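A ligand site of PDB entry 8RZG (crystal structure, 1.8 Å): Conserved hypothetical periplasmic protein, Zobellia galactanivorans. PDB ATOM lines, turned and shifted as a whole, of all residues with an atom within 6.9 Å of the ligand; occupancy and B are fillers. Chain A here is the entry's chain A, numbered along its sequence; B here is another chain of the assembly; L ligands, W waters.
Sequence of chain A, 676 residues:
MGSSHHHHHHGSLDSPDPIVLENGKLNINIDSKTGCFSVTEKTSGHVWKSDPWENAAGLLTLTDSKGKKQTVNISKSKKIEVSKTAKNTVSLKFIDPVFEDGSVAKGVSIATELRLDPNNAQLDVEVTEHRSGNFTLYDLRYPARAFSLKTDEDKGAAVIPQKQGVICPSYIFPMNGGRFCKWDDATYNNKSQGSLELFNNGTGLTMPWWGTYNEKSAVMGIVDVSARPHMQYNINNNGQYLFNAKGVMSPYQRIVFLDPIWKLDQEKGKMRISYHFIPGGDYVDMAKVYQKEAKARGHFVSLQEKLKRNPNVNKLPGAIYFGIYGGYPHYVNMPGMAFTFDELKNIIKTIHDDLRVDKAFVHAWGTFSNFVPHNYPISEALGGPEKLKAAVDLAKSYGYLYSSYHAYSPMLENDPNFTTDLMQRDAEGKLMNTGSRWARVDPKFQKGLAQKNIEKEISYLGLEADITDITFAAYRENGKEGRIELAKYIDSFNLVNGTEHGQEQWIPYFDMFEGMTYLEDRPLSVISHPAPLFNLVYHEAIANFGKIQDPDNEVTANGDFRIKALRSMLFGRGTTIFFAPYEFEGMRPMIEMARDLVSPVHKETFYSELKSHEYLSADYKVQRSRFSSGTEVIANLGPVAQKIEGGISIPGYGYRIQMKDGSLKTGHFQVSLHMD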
ATOM      1  N   TYR A 325      22.580  19.377  16.685  1.00  0.00           N
ATOM      2  CA  TYR A 325      22.608  19.357  15.225  1.00  0.00           C
ATOM      3  C   TYR A 325      23.040  20.729  14.699  1.00  0.00           C
ATOM      4  O   TYR A 325      22.238  21.677  14.702  1.00  0.00           O
ATOM      5  CB  TYR A 325      21.261  18.952  14.634  1.00  0.00           C
ATOM      6  CG  TYR A 325      21.309  18.980  13.126  1.00  0.00           C
ATOM      7  CD1 TYR A 325      21.917  17.951  12.412  1.00  0.00           C
ATOM      8  CD2 TYR A 325      20.812  20.071  12.427  1.00  0.00           C
ATOM      9  CE1 TYR A 325      22.004  17.994  11.026  1.00  0.00           C
ATOM     10  CE2 TYR A 325      20.892  20.127  11.039  1.00  0.00           C
ATOM     11  CZ  TYR A 325      21.489  19.093  10.341  1.00  0.00           C
ATOM     12  OH  TYR A 325      21.579  19.164   8.965  1.00  0.00           O
ATOM     13  N   TYR A 328      25.245  20.180   9.961  1.00  0.00           N
ATOM     14  CA  TYR A 328      26.230  19.250   9.423  1.00  0.00           C
ATOM     15  C   TYR A 328      25.681  17.842   9.586  1.00  0.00           C
ATOM     16  O   TYR A 328      25.132  17.528  10.645  1.00  0.00           O
ATOM     17  CB  TYR A 328      27.554  19.400  10.189  1.00  0.00           C
ATOM     18  CG  TYR A 328      28.764  18.669   9.632  1.00  0.00           C
ATOM     19  CD1 TYR A 328      29.052  17.358  10.000  1.00  0.00           C
ATOM     20  CD2 TYR A 328      29.631  19.305   8.746  1.00  0.00           C
ATOM     21  CE1 TYR A 328      30.172  16.695   9.486  1.00  0.00           C
ATOM     22  CE2 TYR A 328      30.750  18.642   8.233  1.00  0.00           C
ATOM     23  CZ  TYR A 328      31.012  17.341   8.610  1.00  0.00           C
ATOM     24  OH  TYR A 328      32.113  16.685   8.111  1.00  0.00           O
ATOM     25  N   PRO A 329      25.866  16.955   8.606  1.00  0.00           N
ATOM     26  CA  PRO A 329      26.743  16.992   7.424  1.00  0.00           C
ATOM     27  C   PRO A 329      26.215  17.761   6.213  1.00  0.00           C
ATOM     28  O   PRO A 329      26.954  17.901   5.228  1.00  0.00           O
ATOM     29  CB  PRO A 329      26.893  15.508   7.081  1.00  0.00           C
ATOM     30  CG  PRO A 329      25.588  14.916   7.534  1.00  0.00           C
ATOM     31  CD  PRO A 329      25.237  15.634   8.788  1.00  0.00           C
ATOM     32  N   HIS A 330      24.962  18.244   6.296  1.00  0.00           N
ATOM     33  CA  HIS A 330      24.320  18.872   5.151  1.00  0.00           C
ATOM     34  C   HIS A 330      25.051  20.124   4.692  1.00  0.00           C
ATOM     35  O   HIS A 330      25.116  20.412   3.490  1.00  0.00           O
ATOM     36  CB  HIS A 330      22.861  19.193   5.494  1.00  0.00           C
ATOM     37  CG  HIS A 330      22.050  17.983   5.830  1.00  0.00           C
ATOM     38  ND1 HIS A 330      22.227  17.282   7.011  1.00  0.00           N
ATOM     39  CD2 HIS A 330      21.099  17.311   5.131  1.00  0.00           C
ATOM     40  CE1 HIS A 330      21.402  16.245   7.031  1.00  0.00           C
ATOM     41  NE2 HIS A 330      20.709  16.240   5.904  1.00  0.00           N
ATOM     42  N   TRP A 365      26.904  17.139  15.900  1.00  0.00           N
ATOM     43  CA  TRP A 365      26.838  17.097  14.440  1.00  0.00           C
ATOM     44  C   TRP A 365      27.435  18.388  13.884  1.00  0.00           C
ATOM     45  O   TRP A 365      26.740  19.395  13.727  1.00  0.00           O
ATOM     46  CB  TRP A 365      25.408  16.898  13.952  1.00  0.00           C
ATOM     47  CG  TRP A 365      24.782  15.580  14.327  1.00  0.00           C
ATOM     48  CD1 TRP A 365      24.865  14.934  15.531  1.00  0.00           C
ATOM     49  CD2 TRP A 365      23.996  14.736  13.468  1.00  0.00           C
ATOM     50  NE1 TRP A 365      24.158  13.750  15.480  1.00  0.00           N
ATOM     51  CE2 TRP A 365      23.624  13.606  14.223  1.00  0.00           C
ATOM     52  CE3 TRP A 365      23.564  14.842  12.142  1.00  0.00           C
ATOM     53  CZ2 TRP A 365      22.841  12.584  13.695  1.00  0.00           C
ATOM     54  CZ3 TRP A 365      22.789  13.818  11.619  1.00  0.00           C
ATOM     55  CH2 TRP A 365      22.436  12.710  12.395  1.00  0.00           C
ATOM     56  N   TYR A 405      29.821  13.552  14.722  1.00  0.00           N
ATOM     57  CA  TYR A 405      29.115  12.919  13.614  1.00  0.00           C
ATOM     58  C   TYR A 405      30.125  12.411  12.596  1.00  0.00           C
ATOM     59  O   TYR A 405      31.020  13.164  12.198  1.00  0.00           O
ATOM     60  CB  TYR A 405      28.149  13.881  12.929  1.00  0.00           C
ATOM     61  CG  TYR A 405      27.493  13.263  11.710  1.00  0.00           C
ATOM     62  CD1 TYR A 405      28.130  13.270  10.446  1.00  0.00           C
ATOM     63  CD2 TYR A 405      26.262  12.634  11.811  1.00  0.00           C
ATOM     64  CE1 TYR A 405      27.542  12.676   9.347  1.00  0.00           C
ATOM     65  CE2 TYR A 405      25.666  12.042  10.707  1.00  0.00           C
ATOM     66  CZ  TYR A 405      26.303  12.069   9.474  1.00  0.00           C
ATOM     67  OH  TYR A 405      25.684  11.469   8.401  1.00  0.00           O
ATOM     68  N   ALA A 407      30.378   9.956   8.799  1.00  0.00           N
ATOM     69  CA  ALA A 407      29.810   9.100   7.764  1.00  0.00           C
ATOM     70  C   ALA A 407      30.850   8.907   6.670  1.00  0.00           C
ATOM     71  O   ALA A 407      31.549   9.856   6.315  1.00  0.00           O
ATOM     72  CB  ALA A 407      28.519   9.675   7.173  1.00  0.00           C
ATOM     73  N   PRO A 410      28.508   9.100   2.100  1.00  0.00           N
ATOM     74  CA  PRO A 410      27.940  10.133   1.229  1.00  0.00           C
ATOM     75  C   PRO A 410      28.911  10.608   0.170  1.00  0.00           C
ATOM     76  O   PRO A 410      30.134  10.475   0.282  1.00  0.00           O
ATOM     77  CB  PRO A 410      27.587  11.267   2.198  1.00  0.00           C
ATOM     78  CG  PRO A 410      27.589  10.665   3.535  1.00  0.00           C
ATOM     79  CD  PRO A 410      28.630   9.604   3.482  1.00  0.00           C
ATOM     80  N   TRP A 438      23.193  10.255   0.293  1.00  0.00           N
ATOM     81  CA  TRP A 438      23.889   9.887   1.529  1.00  0.00           C
ATOM     82  C   TRP A 438      24.543   8.518   1.460  1.00  0.00           C
ATOM     83  O   TRP A 438      25.369   8.211   2.326  1.00  0.00           O
ATOM     84  CB  TRP A 438      22.924   9.982   2.725  1.00  0.00           C
ATOM     85  CG  TRP A 438      22.528  11.419   2.888  1.00  0.00           C
ATOM     86  CD1 TRP A 438      21.354  11.985   2.519  1.00  0.00           C
ATOM     87  CD2 TRP A 438      23.356  12.479   3.384  1.00  0.00           C
ATOM     88  NE1 TRP A 438      21.379  13.331   2.783  1.00  0.00           N
ATOM     89  CE2 TRP A 438      22.601  13.659   3.298  1.00  0.00           C
ATOM     90  CE3 TRP A 438      24.655  12.545   3.891  1.00  0.00           C
ATOM     91  CZ2 TRP A 438      23.100  14.901   3.711  1.00  0.00           C
ATOM     92  CZ3 TRP A 438      25.154  13.779   4.300  1.00  0.00           C
ATOM     93  CH2 TRP A 438      24.374  14.933   4.202  1.00  0.00           C
ATOM     94  N   ASP A 469      27.190   6.909  10.905  1.00  0.00           N
ATOM     95  CA  ASP A 469      25.840   6.984  10.378  1.00  0.00           C
ATOM     96  C   ASP A 469      25.749   6.339   8.989  1.00  0.00           C
ATOM     97  O   ASP A 469      26.746   6.127   8.305  1.00  0.00           O
ATOM     98  CB  ASP A 469      25.365   8.434  10.323  1.00  0.00           C
ATOM     99  CG  ASP A 469      24.577   8.848  11.563  1.00  0.00           C
ATOM    100  OD1 ASP A 469      25.144   8.827  12.681  1.00  0.00           O
ATOM    101  OD2 ASP A 469      23.390   9.205  11.415  1.00  0.00           O
ATOM    102  N   ILE A 470      24.505   6.002   8.621  1.00  0.00           N
ATOM    103  CA  ILE A 470      24.077   5.554   7.287  1.00  0.00           C
ATOM    104  C   ILE A 470      24.501   4.144   6.898  1.00  0.00           C
ATOM    105  O   ILE A 470      23.641   3.355   6.459  1.00  0.00           O
ATOM    106  CB  ILE A 470      24.536   6.546   6.186  1.00  0.00           C
ATOM    107  CG1 ILE A 470      23.939   7.941   6.431  1.00  0.00           C
ATOM    108  CG2 ILE A 470      24.078   6.059   4.819  1.00  0.00           C
ATOM    109  CD1 ILE A 470      24.768   9.074   5.831  1.00  0.00           C
ATOM    110  N   GLU A 500      23.421   4.456  12.982  1.00  0.00           N
ATOM    111  CA  GLU A 500      22.060   4.828  12.611  1.00  0.00           C
ATOM    112  C   GLU A 500      21.231   3.590  12.277  1.00  0.00           C
ATOM    113  O   GLU A 500      21.627   2.775  11.447  1.00  0.00           O
ATOM    114  CB  GLU A 500      22.065   5.776  11.408  1.00  0.00           C
ATOM    115  CG  GLU A 500      20.659   6.121  10.919  1.00  0.00           C
ATOM    116  CD  GLU A 500      20.631   6.886   9.612  1.00  0.00           C
ATOM    117  OE1 GLU A 500      21.638   6.863   8.876  1.00  0.00           O
ATOM    118  OE2 GLU A 500      19.583   7.515   9.329  1.00  0.00           O
ATOM    119  N   GLU A 514      20.715   3.904  16.839  1.00  0.00           N
ATOM    120  CA  GLU A 514      19.952   5.158  16.846  1.00  0.00           C
ATOM    121  C   GLU A 514      18.765   4.974  15.903  1.00  0.00           C
ATOM    122  O   GLU A 514      18.894   5.090  14.684  1.00  0.00           O
ATOM    123  CB  GLU A 514      20.813   6.346  16.438  1.00  0.00           C
ATOM    124  CG  GLU A 514      20.026   7.635  16.209  1.00  0.00           C
ATOM    125  CD  GLU A 514      19.797   7.931  14.719  1.00  0.00           C
ATOM    126  OE1 GLU A 514      20.760   7.783  13.926  1.00  0.00           O
ATOM    127  OE2 GLU A 514      18.653   8.300  14.352  1.00  0.00           O
ATOM    128  N   LYS A 547      14.857   7.836  16.884  1.00  0.00           N
ATOM    129  CA  LYS A 547      15.447   8.322  15.638  1.00  0.00           C
ATOM    130  C   LYS A 547      15.579   9.846  15.651  1.00  0.00           C
ATOM    131  O   LYS A 547      14.680  10.550  16.109  1.00  0.00           O
ATOM    132  CB  LYS A 547      14.572   7.909  14.447  1.00  0.00           C
ATOM    133  CG  LYS A 547      15.258   8.031  13.088  1.00  0.00           C
ATOM    134  CD  LYS A 547      16.265   6.891  12.911  1.00  0.00           C
ATOM    135  CE  LYS A 547      17.003   6.972  11.564  1.00  0.00           C
ATOM    136  NZ  LYS A 547      17.920   8.151  11.512  1.00  0.00           N
ATOM    137  N   ILE A 548      16.687  10.347  15.092  1.00  0.00           N
ATOM    138  CA  ILE A 548      16.948  11.788  15.149  1.00  0.00           C
ATOM    139  C   ILE A 548      15.944  12.580  14.297  1.00  0.00           C
ATOM    140  O   ILE A 548      15.689  13.762  14.589  1.00  0.00           O
ATOM    141  CB  ILE A 548      18.412  12.100  14.743  1.00  0.00           C
ATOM    142  CG1 ILE A 548      18.701  11.636  13.314  1.00  0.00           C
ATOM    143  CG2 ILE A 548      19.412  11.473  15.729  1.00  0.00           C
ATOM    144  CD1 ILE A 548      18.730  12.763  12.284  1.00  0.00           C
ATOM    145  N   GLN A 549      15.373  11.987  13.249  1.00  0.00           N
ATOM    146  CA  GLN A 549      14.360  12.709  12.472  1.00  0.00           C
ATOM    147  C   GLN A 549      13.041  12.846  13.219  1.00  0.00           C
ATOM    148  O   GLN A 549      12.246  13.729  12.902  1.00  0.00           O
ATOM    149  CB  GLN A 549      14.076  12.023  11.134  1.00  0.00           C
ATOM    150  CG  GLN A 549      15.110  12.287  10.019  1.00  0.00           C
ATOM    151  CD  GLN A 549      16.278  11.340  10.118  1.00  0.00           C
ATOM    152  OE1 GLN A 549      16.370  10.554  11.058  1.00  0.00           O
ATOM    153  NE2 GLN A 549      17.190  11.393   9.144  1.00  0.00           N
ATOM    154  N   PHE A 578      17.048  15.753  20.184  1.00  0.00           N
ATOM    155  CA  PHE A 578      17.783  16.098  18.964  1.00  0.00           C
ATOM    156  C   PHE A 578      17.365  17.486  18.512  1.00  0.00           C
ATOM    157  O   PHE A 578      16.193  17.709  18.171  1.00  0.00           O
ATOM    158  CB  PHE A 578      17.536  15.061  17.868  1.00  0.00           C
ATOM    159  CG  PHE A 578      18.491  15.180  16.703  1.00  0.00           C
ATOM    160  CD1 PHE A 578      19.779  14.660  16.800  1.00  0.00           C
ATOM    161  CD2 PHE A 578      18.114  15.831  15.541  1.00  0.00           C
ATOM    162  CE1 PHE A 578      20.680  14.784  15.724  1.00  0.00           C
ATOM    163  CE2 PHE A 578      19.014  15.945  14.462  1.00  0.00           C
ATOM    164  CZ  PHE A 578      20.290  15.421  14.574  1.00  0.00           C
ATOM    165  N   PHE B 180      15.154  19.594   9.887  1.00  0.00           N
ATOM    166  CA  PHE B 180      16.137  20.088   8.917  1.00  0.00           C
ATOM    167  C   PHE B 180      16.625  18.960   8.010  1.00  0.00           C
ATOM    168  O   PHE B 180      16.727  19.134   6.788  1.00  0.00           O
ATOM    169  CB  PHE B 180      17.301  20.715   9.683  1.00  0.00           C
ATOM    170  CG  PHE B 180      18.252  21.522   8.833  1.00  0.00           C
ATOM    171  CD1 PHE B 180      19.168  20.885   8.014  1.00  0.00           C
ATOM    172  CD2 PHE B 180      18.265  22.902   8.920  1.00  0.00           C
ATOM    173  CE1 PHE B 180      20.067  21.614   7.243  1.00  0.00           C
ATOM    174  CE2 PHE B 180      19.158  23.652   8.152  1.00  0.00           C
ATOM    175  CZ  PHE B 180      20.064  23.000   7.321  1.00  0.00           C
ATOM    176  N   CYS B 181      16.973  17.813   8.585  1.00  0.00           N
ATOM    177  CA  CYS B 181      17.454  16.688   7.788  1.00  0.00           C
ATOM    178  C   CYS B 181      16.403  16.251   6.767  1.00  0.00           C
ATOM    179  O   CYS B 181      16.719  16.077   5.585  1.00  0.00           O
ATOM    180  CB  CYS B 181      17.858  15.511   8.687  1.00  0.00           C
ATOM    181  SG  CYS B 181      19.285  15.800   9.772  1.00  0.00           S
ATOM    182  N   LYS B 182      15.153  16.082   7.220  1.00  0.00           N
ATOM    183  CA  LYS B 182      14.087  15.674   6.298  1.00  0.00           C
ATOM    184  C   LYS B 182      13.854  16.738   5.223  1.00  0.00           C
ATOM    185  O   LYS B 182      13.628  16.410   4.059  1.00  0.00           O
ATOM    186  CB  LYS B 182      12.782  15.416   7.066  1.00  0.00           C
ATOM    187  CG  LYS B 182      12.776  14.169   7.976  1.00  0.00           C
ATOM    188  CD  LYS B 182      11.397  13.962   8.654  1.00  0.00           C
ATOM    189  CE  LYS B 182      11.204  14.915   9.838  1.00  0.00           C
ATOM    190  NZ  LYS B 182       9.932  14.625  10.595  1.00  0.00           N
ATOM    191  N   ASP B 185      16.964  16.862   2.703  1.00  0.00           N
ATOM    192  CA  ASP B 185      17.027  15.622   1.924  1.00  0.00           C
ATOM    193  C   ASP B 185      15.936  15.579   0.864  1.00  0.00           C
ATOM    194  O   ASP B 185      16.156  15.044  -0.241  1.00  0.00           O
ATOM    195  CB  ASP B 185      16.895  14.403   2.853  1.00  0.00           C
ATOM    196  CG  ASP B 185      18.124  14.198   3.737  1.00  0.00           C
ATOM    197  OD1 ASP B 185      19.052  15.025   3.677  1.00  0.00           O
ATOM    198  OD2 ASP B 185      18.133  13.206   4.505  1.00  0.00           O
HETATM  199  C1  LIG L   1      22.461  10.385   8.598  1.00  0.00           C
HETATM  200  C2  LIG L   1      21.229  11.241   9.315  1.00  0.00           C
HETATM  201  C3  LIG L   1      20.858  12.431   8.545  1.00  0.00           C
HETATM  202  C4  LIG L   1      20.482  12.134   7.307  1.00  0.00           C
HETATM  203  C5  LIG L   1      21.509  11.662   6.592  1.00  0.00           C
HETATM  204  C6  LIG L   1      22.545  12.705   6.904  1.00  0.00           C
HETATM  205  O1  LIG L   1      21.982  10.374   7.050  1.00  0.00           O
HETATM  206  O2  LIG L   1      20.078  10.446   9.260  1.00  0.00           O
HETATM  207  O3  LIG L   1      22.077  13.238   8.285  1.00  0.00           O
HETATM  208  O4  LIG L   1      19.887  13.269   6.689  1.00  0.00           O
HETATM  209  O   HOH W   1      16.517  12.862   6.776  1.00  0.00           O
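O4 of the ligand lies within hydrogen-bond range of OD2 of Asp 185 of chain B, at 2.8 Å. The side-chain carboxylate (OE2) of Glu 500 is in hydrogen-bond range of an oxygen (O2) of the ligand (3.0 Å). NE2 of Gln 549 lies within hydrogen-bond range of O2 of the ligand (3.0 Å). A ring nitrogen (NE2) of His 330 is in hydrogen-bond range of an oxygen (O4) of the ligand, at 3.2 Å.
A ring nitrogen (NE2) of His 330 sits at hydrogen-bond distance from the side-chain carboxylate of Asp 185 of chain B (3.0 Å). The indole nitrogen of Trp 438 sits at hydrogen-bond distance from the side-chain carboxylate of Asp 185 of chain B, 3.0 Å away. The side-chain carboxylate of Glu 500 is in hydrogen-bond range of the backbone NH of Ile 470 (3.0 Å). OE2 of Glu 500 lies within salt-bridge range of NZ of Lys 547, 2.8 Å away. The side-chain amino group (NZ) of Lys 547 is in hydrogen-bond range of the side-chain amide oxygen (OE1) of Gln 549 (2.9 Å). NZ of Lys 182 of chain B is in hydrogen-bond range of O of Gln 549, 3.4 Å away. OH of Tyr 325 is in hydrogen-bond range of ND1 of His 330, at 2.8 Å. OE2 of Glu 514 is in salt-bridge range of NZ of Lys 547, 2.9 Å away.
Merely in contact with the ligand: Ile 470 (3.2 Å), Asp 469 (3.2 Å), Tyr 405 (3.4 Å), Trp 365 (3.5 Å), Trp 438 (3.6 Å), Cys 181 of chain B (3.6 Å), Pro 329 (3.8 Å) and Lys 547 (3.9 Å). Hydrophobic or aromatic side chains within 4 Å of the ligand: Pro 329, His 330, Trp 365, Trp 438 and Ile 470. Within 4 Å of the ligand: Pro 329, His 330, Trp 365, Tyr 405, Trp 438, Asp 469, Ile 470, Glu 500, Lys 547, Gln 549, Cys 181 of chain B and Asp 185 of chain B. Along chain A the residues within 4 Å of the ligand span positions 329 to 549.
Water W1 lies within hydrogen-bond range of the side-chain carboxylate of Asp 185 of chain B (2.8 Å), the side-chain amide nitrogen of Gln 549 (2.9 Å), an oxygen (O4) of the ligand (3.4 Å) and the backbone carbonyl oxygen of Cys 181 of chain B (3.4 Å).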
